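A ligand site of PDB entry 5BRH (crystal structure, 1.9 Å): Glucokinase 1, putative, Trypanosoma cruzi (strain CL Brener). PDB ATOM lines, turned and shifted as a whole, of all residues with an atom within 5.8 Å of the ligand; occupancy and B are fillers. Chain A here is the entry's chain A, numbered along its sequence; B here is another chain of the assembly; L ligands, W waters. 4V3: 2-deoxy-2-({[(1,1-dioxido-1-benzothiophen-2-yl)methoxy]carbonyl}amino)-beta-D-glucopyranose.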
ATOM      1  N   VAL A 105       4.289   6.636 -15.559  1.00  0.00           N
ATOM      2  CA  VAL A 105       5.574   6.835 -16.216  1.00  0.00           C
ATOM      3  C   VAL A 105       5.404   7.428 -17.628  1.00  0.00           C
ATOM      4  O   VAL A 105       4.352   7.257 -18.252  1.00  0.00           O
ATOM      5  CB  VAL A 105       6.347   5.512 -16.309  1.00  0.00           C
ATOM      6  CG1 VAL A 105       6.611   4.989 -14.925  1.00  0.00           C
ATOM      7  CG2 VAL A 105       5.545   4.494 -17.090  1.00  0.00           C
ATOM      8  N   PRO A 106       6.429   8.135 -18.132  1.00  0.00           N
ATOM      9  CA  PRO A 106       6.239   8.847 -19.403  1.00  0.00           C
ATOM     10  C   PRO A 106       6.458   7.996 -20.649  1.00  0.00           C
ATOM     11  O   PRO A 106       7.154   8.432 -21.571  1.00  0.00           O
ATOM     12  CB  PRO A 106       7.302   9.944 -19.330  1.00  0.00           C
ATOM     13  CG  PRO A 106       8.409   9.318 -18.562  1.00  0.00           C
ATOM     14  CD  PRO A 106       7.718   8.466 -17.506  1.00  0.00           C
ATOM     15  N   GLY A 107       5.864   6.806 -20.706  1.00  0.00           N
ATOM     16  CA  GLY A 107       5.974   5.961 -21.881  1.00  0.00           C
ATOM     17  C   GLY A 107       4.895   4.896 -21.842  1.00  0.00           C
ATOM     18  O   GLY A 107       4.129   4.833 -20.889  1.00  0.00           O
ATOM     19  N   PRO A 108       4.834   4.046 -22.887  1.00  0.00           N
ATOM     20  CA  PRO A 108       3.762   3.032 -22.963  1.00  0.00           C
ATOM     21  C   PRO A 108       3.884   2.028 -21.818  1.00  0.00           C
ATOM     22  O   PRO A 108       5.007   1.701 -21.403  1.00  0.00           O
ATOM     23  CB  PRO A 108       4.043   2.317 -24.296  1.00  0.00           C
ATOM     24  CG  PRO A 108       4.960   3.242 -25.074  1.00  0.00           C
ATOM     25  CD  PRO A 108       5.748   3.986 -24.041  1.00  0.00           C
ATOM     26  N   PRO A 117      10.081   0.944 -23.207  1.00  0.00           N
ATOM     27  CA  PRO A 117      11.185   1.851 -22.877  1.00  0.00           C
ATOM     28  C   PRO A 117      10.773   3.317 -23.012  1.00  0.00           C
ATOM     29  O   PRO A 117       9.722   3.635 -23.599  1.00  0.00           O
ATOM     30  CB  PRO A 117      12.266   1.510 -23.924  1.00  0.00           C
ATOM     31  CG  PRO A 117      11.663   0.418 -24.820  1.00  0.00           C
ATOM     32  CD  PRO A 117      10.178   0.435 -24.579  1.00  0.00           C
ATOM     33  N   PHE A 118      11.583   4.202 -22.461  1.00  0.00           N
ATOM     34  CA  PHE A 118      11.269   5.615 -22.486  1.00  0.00           C
ATOM     35  C   PHE A 118      12.292   6.350 -23.333  1.00  0.00           C
ATOM     36  O   PHE A 118      13.435   5.904 -23.470  1.00  0.00           O
ATOM     37  CB  PHE A 118      11.253   6.162 -21.058  1.00  0.00           C
ATOM     38  CG  PHE A 118      10.409   5.341 -20.129  1.00  0.00           C
ATOM     39  CD1 PHE A 118       9.031   5.448 -20.164  1.00  0.00           C
ATOM     40  CD2 PHE A 118      11.001   4.454 -19.236  1.00  0.00           C
ATOM     41  CE1 PHE A 118       8.236   4.685 -19.319  1.00  0.00           C
ATOM     42  CE2 PHE A 118      10.218   3.683 -18.382  1.00  0.00           C
ATOM     43  CZ  PHE A 118       8.834   3.802 -18.418  1.00  0.00           C
ATOM     44  N   ASN A 119      11.900   7.464 -23.933  1.00  0.00           N
ATOM     45  CA  ASN A 119      12.838   8.171 -24.800  1.00  0.00           C
ATOM     46  C   ASN A 119      13.681   9.207 -24.055  1.00  0.00           C
ATOM     47  O   ASN A 119      14.563   9.826 -24.643  1.00  0.00           O
ATOM     48  CB  ASN A 119      12.131   8.760 -26.015  1.00  0.00           C
ATOM     49  CG  ASN A 119      11.716  10.194 -25.814  1.00  0.00           C
ATOM     50  OD1 ASN A 119      11.064  10.526 -24.823  1.00  0.00           O
ATOM     51  ND2 ASN A 119      12.076  11.061 -26.767  1.00  0.00           N
ATOM     52  N   ASN A 144       0.412   4.607 -17.799  1.00  0.00           N
ATOM     53  CA  ASN A 144       0.992   5.598 -18.697  1.00  0.00           C
ATOM     54  C   ASN A 144       0.618   6.991 -18.162  1.00  0.00           C
ATOM     55  O   ASN A 144      -0.449   7.162 -17.552  1.00  0.00           O
ATOM     56  CB  ASN A 144       0.472   5.344 -20.104  1.00  0.00           C
ATOM     57  CG  ASN A 144       0.697   6.517 -21.044  1.00  0.00           C
ATOM     58  OD1 ASN A 144      -0.185   7.358 -21.224  1.00  0.00           O
ATOM     59  ND2 ASN A 144       1.857   6.542 -21.685  1.00  0.00           N
ATOM     60  N   ASP A 145       1.490   7.987 -18.339  1.00  0.00           N
ATOM     61  CA  ASP A 145       1.200   9.327 -17.825  1.00  0.00           C
ATOM     62  C   ASP A 145      -0.152   9.900 -18.265  1.00  0.00           C
ATOM     63  O   ASP A 145      -0.852  10.498 -17.444  1.00  0.00           O
ATOM     64  CB  ASP A 145       2.350  10.314 -18.097  1.00  0.00           C
ATOM     65  CG  ASP A 145       2.636  10.521 -19.578  1.00  0.00           C
ATOM     66  OD1 ASP A 145       2.157   9.728 -20.417  1.00  0.00           O
ATOM     67  OD2 ASP A 145       3.390  11.476 -19.914  1.00  0.00           O
ATOM     68  N   LEU A 146      -0.542   9.700 -19.528  1.00  0.00           N
ATOM     69  CA  LEU A 146      -1.828  10.244 -19.975  1.00  0.00           C
ATOM     70  C   LEU A 146      -2.980   9.310 -19.610  1.00  0.00           C
ATOM     71  O   LEU A 146      -4.132   9.736 -19.573  1.00  0.00           O
ATOM     72  CB  LEU A 146      -1.833  10.564 -21.473  1.00  0.00           C
ATOM     73  CG  LEU A 146      -1.557  12.036 -21.743  1.00  0.00           C
ATOM     74  CD1 LEU A 146      -2.730  12.872 -21.200  1.00  0.00           C
ATOM     75  CD2 LEU A 146      -0.264  12.469 -21.060  1.00  0.00           C
ATOM     76  N   ALA A 196      -2.244  15.995 -24.478  1.00  0.00           N
ATOM     77  CA  ALA A 196      -1.317  16.769 -23.667  1.00  0.00           C
ATOM     78  C   ALA A 196      -0.072  17.095 -24.465  1.00  0.00           C
ATOM     79  O   ALA A 196       0.877  16.328 -24.502  1.00  0.00           O
ATOM     80  CB  ALA A 196      -0.927  16.006 -22.407  1.00  0.00           C
ATOM     81  N   GLY A 200       6.651  15.496 -24.767  1.00  0.00           N
ATOM     82  CA  GLY A 200       6.108  14.617 -25.781  1.00  0.00           C
ATOM     83  C   GLY A 200       4.632  14.917 -25.945  1.00  0.00           C
ATOM     84  O   GLY A 200       4.037  15.639 -25.132  1.00  0.00           O
ATOM     85  N   LEU A 201       4.020  14.375 -26.991  1.00  0.00           N
ATOM     86  CA  LEU A 201       2.596  14.579 -27.201  1.00  0.00           C
ATOM     87  C   LEU A 201       1.832  13.391 -26.620  1.00  0.00           C
ATOM     88  O   LEU A 201       1.907  12.281 -27.162  1.00  0.00           O
ATOM     89  CB  LEU A 201       2.277  14.740 -28.689  1.00  0.00           C
ATOM     90  CG  LEU A 201       0.798  14.760 -29.080  1.00  0.00           C
ATOM     91  CD1 LEU A 201       0.083  15.890 -28.357  1.00  0.00           C
ATOM     92  CD2 LEU A 201       0.661  14.914 -30.611  1.00  0.00           C
ATOM     93  N   GLY A 202       1.104  13.627 -25.538  1.00  0.00           N
ATOM     94  CA  GLY A 202       0.378  12.551 -24.889  1.00  0.00           C
ATOM     95  C   GLY A 202      -1.073  12.463 -25.316  1.00  0.00           C
ATOM     96  O   GLY A 202      -1.677  13.471 -25.691  1.00  0.00           O
ATOM     97  N   SER A 203      -1.647  11.261 -25.240  1.00  0.00           N
ATOM     98  CA  SER A 203      -3.036  11.081 -25.619  1.00  0.00           C
ATOM     99  C   SER A 203      -3.654   9.891 -24.881  1.00  0.00           C
ATOM    100  O   SER A 203      -3.006   8.858 -24.718  1.00  0.00           O
ATOM    101  CB  SER A 203      -3.155  10.842 -27.113  1.00  0.00           C
ATOM    102  OG  SER A 203      -2.389   9.713 -27.526  1.00  0.00           O
ATOM    103  N   LEU A 220      -3.413   5.690 -25.358  1.00  0.00           N
ATOM    104  CA  LEU A 220      -3.222   5.757 -26.793  1.00  0.00           C
ATOM    105  C   LEU A 220      -1.807   6.259 -27.053  1.00  0.00           C
ATOM    106  O   LEU A 220      -1.184   6.813 -26.148  1.00  0.00           O
ATOM    107  CB  LEU A 220      -4.216   6.755 -27.399  1.00  0.00           C
ATOM    108  CG  LEU A 220      -5.718   6.500 -27.273  1.00  0.00           C
ATOM    109  CD1 LEU A 220      -6.468   7.692 -27.895  1.00  0.00           C
ATOM    110  CD2 LEU A 220      -6.115   5.203 -27.955  1.00  0.00           C
ATOM    111  N   GLU A 221      -1.328   6.075 -28.283  1.00  0.00           N
ATOM    112  CA  GLU A 221      -0.067   6.668 -28.732  1.00  0.00           C
ATOM    113  C   GLU A 221      -0.311   7.406 -30.040  1.00  0.00           C
ATOM    114  O   GLU A 221       0.324   7.142 -31.061  1.00  0.00           O
ATOM    115  CB  GLU A 221       1.011   5.586 -28.941  1.00  0.00           C
ATOM    116  CG  GLU A 221       1.452   4.910 -27.612  1.00  0.00           C
ATOM    117  CD  GLU A 221       2.261   5.835 -26.745  1.00  0.00           C
ATOM    118  OE1 GLU A 221       2.863   6.784 -27.296  1.00  0.00           O
ATOM    119  OE2 GLU A 221       2.316   5.616 -25.503  1.00  0.00           O
ATOM    120  N   SER A 224       2.579   9.264 -32.186  1.00  0.00           N
ATOM    121  CA  SER A 224       3.554   8.544 -33.014  1.00  0.00           C
ATOM    122  C   SER A 224       2.998   8.086 -34.363  1.00  0.00           C
ATOM    123  O   SER A 224       3.691   7.396 -35.103  1.00  0.00           O
ATOM    124  CB  SER A 224       4.160   7.387 -32.221  1.00  0.00           C
ATOM    125  OG  SER A 224       4.883   7.896 -31.109  1.00  0.00           O
ATOM    126  N   GLU A 250       3.911  14.057 -33.109  1.00  0.00           N
ATOM    127  CA  GLU A 250       4.805  14.552 -32.080  1.00  0.00           C
ATOM    128  C   GLU A 250       5.991  15.368 -32.637  1.00  0.00           C
ATOM    129  O   GLU A 250       6.453  16.314 -31.992  1.00  0.00           O
ATOM    130  CB  GLU A 250       5.331  13.407 -31.213  1.00  0.00           C
ATOM    131  CG  GLU A 250       6.099  13.891 -30.005  1.00  0.00           C
ATOM    132  CD  GLU A 250       6.483  12.723 -29.109  1.00  0.00           C
ATOM    133  OE1 GLU A 250       7.469  12.015 -29.438  1.00  0.00           O
ATOM    134  OE2 GLU A 250       5.788  12.502 -28.099  1.00  0.00           O
ATOM    135  N   MET B 309       0.550   1.322 -33.876  1.00  0.00           N
ATOM    136  CA  MET B 309       1.165   2.320 -33.037  1.00  0.00           C
ATOM    137  C   MET B 309       0.152   3.033 -32.155  1.00  0.00           C
ATOM    138  O   MET B 309       0.307   3.103 -30.922  1.00  0.00           O
ATOM    139  CB  MET B 309       1.939   3.340 -33.912  1.00  0.00           C
ATOM    140  CG  MET B 309       2.810   4.277 -33.080  1.00  0.00           C
ATOM    141  SD  MET B 309       4.113   3.376 -32.226  1.00  0.00           S
ATOM    142  CE  MET B 309       3.763   3.775 -30.509  1.00  0.00           C
ATOM    143  N   MET B 348       8.152   3.705 -36.536  1.00  0.00           N
ATOM    144  CA  MET B 348       8.261   3.271 -35.136  1.00  0.00           C
ATOM    145  C   MET B 348       8.656   1.809 -35.042  1.00  0.00           C
ATOM    146  O   MET B 348       8.886   1.302 -33.950  1.00  0.00           O
ATOM    147  CB  MET B 348       6.958   3.516 -34.385  1.00  0.00           C
ATOM    148  CG  MET B 348       6.569   4.985 -34.319  1.00  0.00           C
ATOM    149  SD  MET B 348       7.761   5.944 -33.368  1.00  0.00           S
ATOM    150  CE  MET B 348       7.348   5.447 -31.704  1.00  0.00           C
ATOM    151  N   ARG B 350      11.433   0.812 -35.910  1.00  0.00           N
ATOM    152  CA  ARG B 350      12.811   0.858 -35.442  1.00  0.00           C
ATOM    153  C   ARG B 350      12.874   0.552 -33.937  1.00  0.00           C
ATOM    154  O   ARG B 350      13.920   0.146 -33.424  1.00  0.00           O
ATOM    155  CB  ARG B 350      13.501   2.194 -35.792  1.00  0.00           C
ATOM    156  CG  ARG B 350      13.166   3.390 -34.868  1.00  0.00           C
ATOM    157  CD  ARG B 350      13.645   4.697 -35.537  1.00  0.00           C
ATOM    158  NE  ARG B 350      13.468   5.866 -34.683  1.00  0.00           N
ATOM    159  CZ  ARG B 350      12.349   6.588 -34.627  1.00  0.00           C
ATOM    160  NH1 ARG B 350      11.299   6.243 -35.371  1.00  0.00           N
ATOM    161  NH2 ARG B 350      12.261   7.639 -33.822  1.00  0.00           N
ATOM    162  N   PHE B 351      11.748   0.723 -33.248  1.00  0.00           N
ATOM    163  CA  PHE B 351      11.644   0.300 -31.850  1.00  0.00           C
ATOM    164  C   PHE B 351      10.817  -0.990 -31.656  1.00  0.00           C
ATOM    165  O   PHE B 351      10.517  -1.390 -30.519  1.00  0.00           O
ATOM    166  CB  PHE B 351      11.014   1.427 -31.017  1.00  0.00           C
ATOM    167  CG  PHE B 351      11.726   2.755 -31.188  1.00  0.00           C
ATOM    168  CD1 PHE B 351      13.062   2.882 -30.840  1.00  0.00           C
ATOM    169  CD2 PHE B 351      11.031   3.868 -31.660  1.00  0.00           C
ATOM    170  CE1 PHE B 351      13.723   4.107 -30.984  1.00  0.00           C
ATOM    171  CE2 PHE B 351      11.681   5.105 -31.789  1.00  0.00           C
ATOM    172  CZ  PHE B 351      13.032   5.213 -31.469  1.00  0.00           C
ATOM    173  N   PHE B 353       7.617  -1.587 -32.580  1.00  0.00           N
ATOM    174  CA  PHE B 353       6.194  -1.476 -32.254  1.00  0.00           C
ATOM    175  C   PHE B 353       5.288  -2.301 -33.148  1.00  0.00           C
ATOM    176  O   PHE B 353       4.352  -2.915 -32.653  1.00  0.00           O
ATOM    177  CB  PHE B 353       5.718  -0.010 -32.166  1.00  0.00           C
ATOM    178  CG  PHE B 353       6.079   0.648 -30.872  1.00  0.00           C
ATOM    179  CD1 PHE B 353       5.352   0.366 -29.712  1.00  0.00           C
ATOM    180  CD2 PHE B 353       7.166   1.520 -30.772  1.00  0.00           C
ATOM    181  CE1 PHE B 353       5.673   0.965 -28.494  1.00  0.00           C
ATOM    182  CE2 PHE B 353       7.509   2.114 -29.554  1.00  0.00           C
ATOM    183  CZ  PHE B 353       6.767   1.847 -28.416  1.00  0.00           C
HETATM  184  C10 4V3 L   1       3.526  12.183 -23.128  1.00  0.00           C
HETATM  185  C13 4V3 L   1       6.523   6.955 -26.159  1.00  0.00           C
HETATM  186  C01 4V3 L   1       3.813   8.600 -24.561  1.00  0.00           C
HETATM  187  C02 4V3 L   1       5.198   8.797 -25.183  1.00  0.00           C
HETATM  188  C03 4V3 L   1       5.243  10.214 -25.784  1.00  0.00           C
HETATM  189  O04 4V3 L   1       5.113  11.137 -24.705  1.00  0.00           O
HETATM  190  C05 4V3 L   1       3.752  11.051 -24.146  1.00  0.00           C
HETATM  191  C06 4V3 L   1       3.555   9.669 -23.521  1.00  0.00           C
HETATM  192  N07 4V3 L   1       5.411   7.732 -26.170  1.00  0.00           N
HETATM  193  O08 4V3 L   1       2.202   9.597 -23.037  1.00  0.00           O
HETATM  194  O09 4V3 L   1       3.777   7.268 -23.951  1.00  0.00           O
HETATM  195  O11 4V3 L   1       6.370  10.445 -26.425  1.00  0.00           O
HETATM  196  O12 4V3 L   1       4.546  12.143 -22.126  1.00  0.00           O
HETATM  197  O14 4V3 L   1       6.550   6.063 -27.182  1.00  0.00           O
HETATM  198  O15 4V3 L   1       7.509   7.178 -25.449  1.00  0.00           O
HETATM  199  C16 4V3 L   1       7.725   5.302 -27.284  1.00  0.00           C
HETATM  200  C17 4V3 L   1       8.905   6.129 -27.867  1.00  0.00           C
HETATM  201  C18 4V3 L   1       8.871   7.144 -28.731  1.00  0.00           C
HETATM  202  C19 4V3 L   1      10.185   7.642 -29.099  1.00  0.00           C
HETATM  203  C20 4V3 L   1      11.223   6.823 -28.637  1.00  0.00           C
HETATM  204  S21 4V3 L   1      10.541   5.470 -27.736  1.00  0.00           S
HETATM  205  C22 4V3 L   1      10.517   8.780 -29.853  1.00  0.00           C
HETATM  206  C23 4V3 L   1      11.835   9.114 -30.117  1.00  0.00           C
HETATM  207  C24 4V3 L   1      12.880   8.284 -29.630  1.00  0.00           C
HETATM  208  C25 4V3 L   1      12.561   7.143 -28.896  1.00  0.00           C
HETATM  209  O26 4V3 L   1      10.958   5.463 -26.353  1.00  0.00           O
HETATM  210  O27 4V3 L   1      10.640   4.218 -28.438  1.00  0.00           O
HETATM  211  O   HOH W   1       0.215   9.100 -24.924  1.00  0.00           O
HETATM  212  O   HOH W   2       5.348  14.977 -22.352  1.00  0.00           O
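The side-chain carboxylate (OD2) of Asp 145 lies within hydrogen-bond range of an oxygen (O12) of the ligand (2.6 Å). The side-chain carboxylate (OE2) of Glu 221 lies within hydrogen-bond range of an oxygen (O09) of the ligand, 2.7 Å away. O11 of the ligand is in hydrogen-bond range of OE2 of Glu 250, 2.7 Å away. O09 of the ligand is in hydrogen-bond range of ND2 of Asn 144 (3.1 Å). N of Asn 119 is in hydrogen-bond range of O26 of the ligand, at 3.3 Å.
The side-chain carboxylate (OD1) of Asp 145 sits close to the side-chain amide oxygen (OD1) of Asn 144, 3.4 Å away. The backbone NH of Asp 145 is in hydrogen-bond range of the backbone carbonyl oxygen of Val 105, 3.0 Å away. The backbone NH of Leu 201 sits at hydrogen-bond distance from the side-chain carboxylate of Glu 250 (2.8 Å). ND2 of Asn 144 sits at hydrogen-bond distance from O of Gly 107, 3.0 Å away. The side-chain amide oxygen (OD1) of Asn 144 sits at hydrogen-bond distance from the backbone NH (N) of Leu 146 (2.9 Å). The backbone carbonyl oxygen (O) of Gly 202 lies within hydrogen-bond range of the backbone NH (N) of Ala 196 (2.9 Å). The backbone carbonyl oxygen (O) of Met 348 of chain B sits at hydrogen-bond distance from the backbone NH (N) of Phe 353 of chain B (3.4 Å).
Merely in contact with the ligand: Gly 107 (3.3 Å), Pro 108 (3.6 Å), Pro 117 (3.5 Å), Phe 118 (3.4 Å), Gly 200 (3.8 Å), Leu 201 (3.7 Å), Gly 202 (3.6 Å), Met 348 of chain B (3.7 Å), Phe 351 of chain B (3.3 Å) and Phe 353 of chain B (3.8 Å). 15 residues have an atom within 4 Å of the ligand: Gly 107, Pro 108, Pro 117, Phe 118, Asn 119, Asn 144, Asp 145, Gly 200, Leu 201, Gly 202, Glu 221, Glu 250, Met 348 of chain B, Phe 351 of chain B and Phe 353 of chain B.
Water W1 lies within hydrogen-bond range of O08 of the ligand (2.8 Å), N of Ser 203 (2.9 Å) and O of Leu 220 (2.9 Å). Water W2 lies within hydrogen-bond range of N of Gly 200 (2.8 Å) and O12 of the ligand (3.0 Å).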
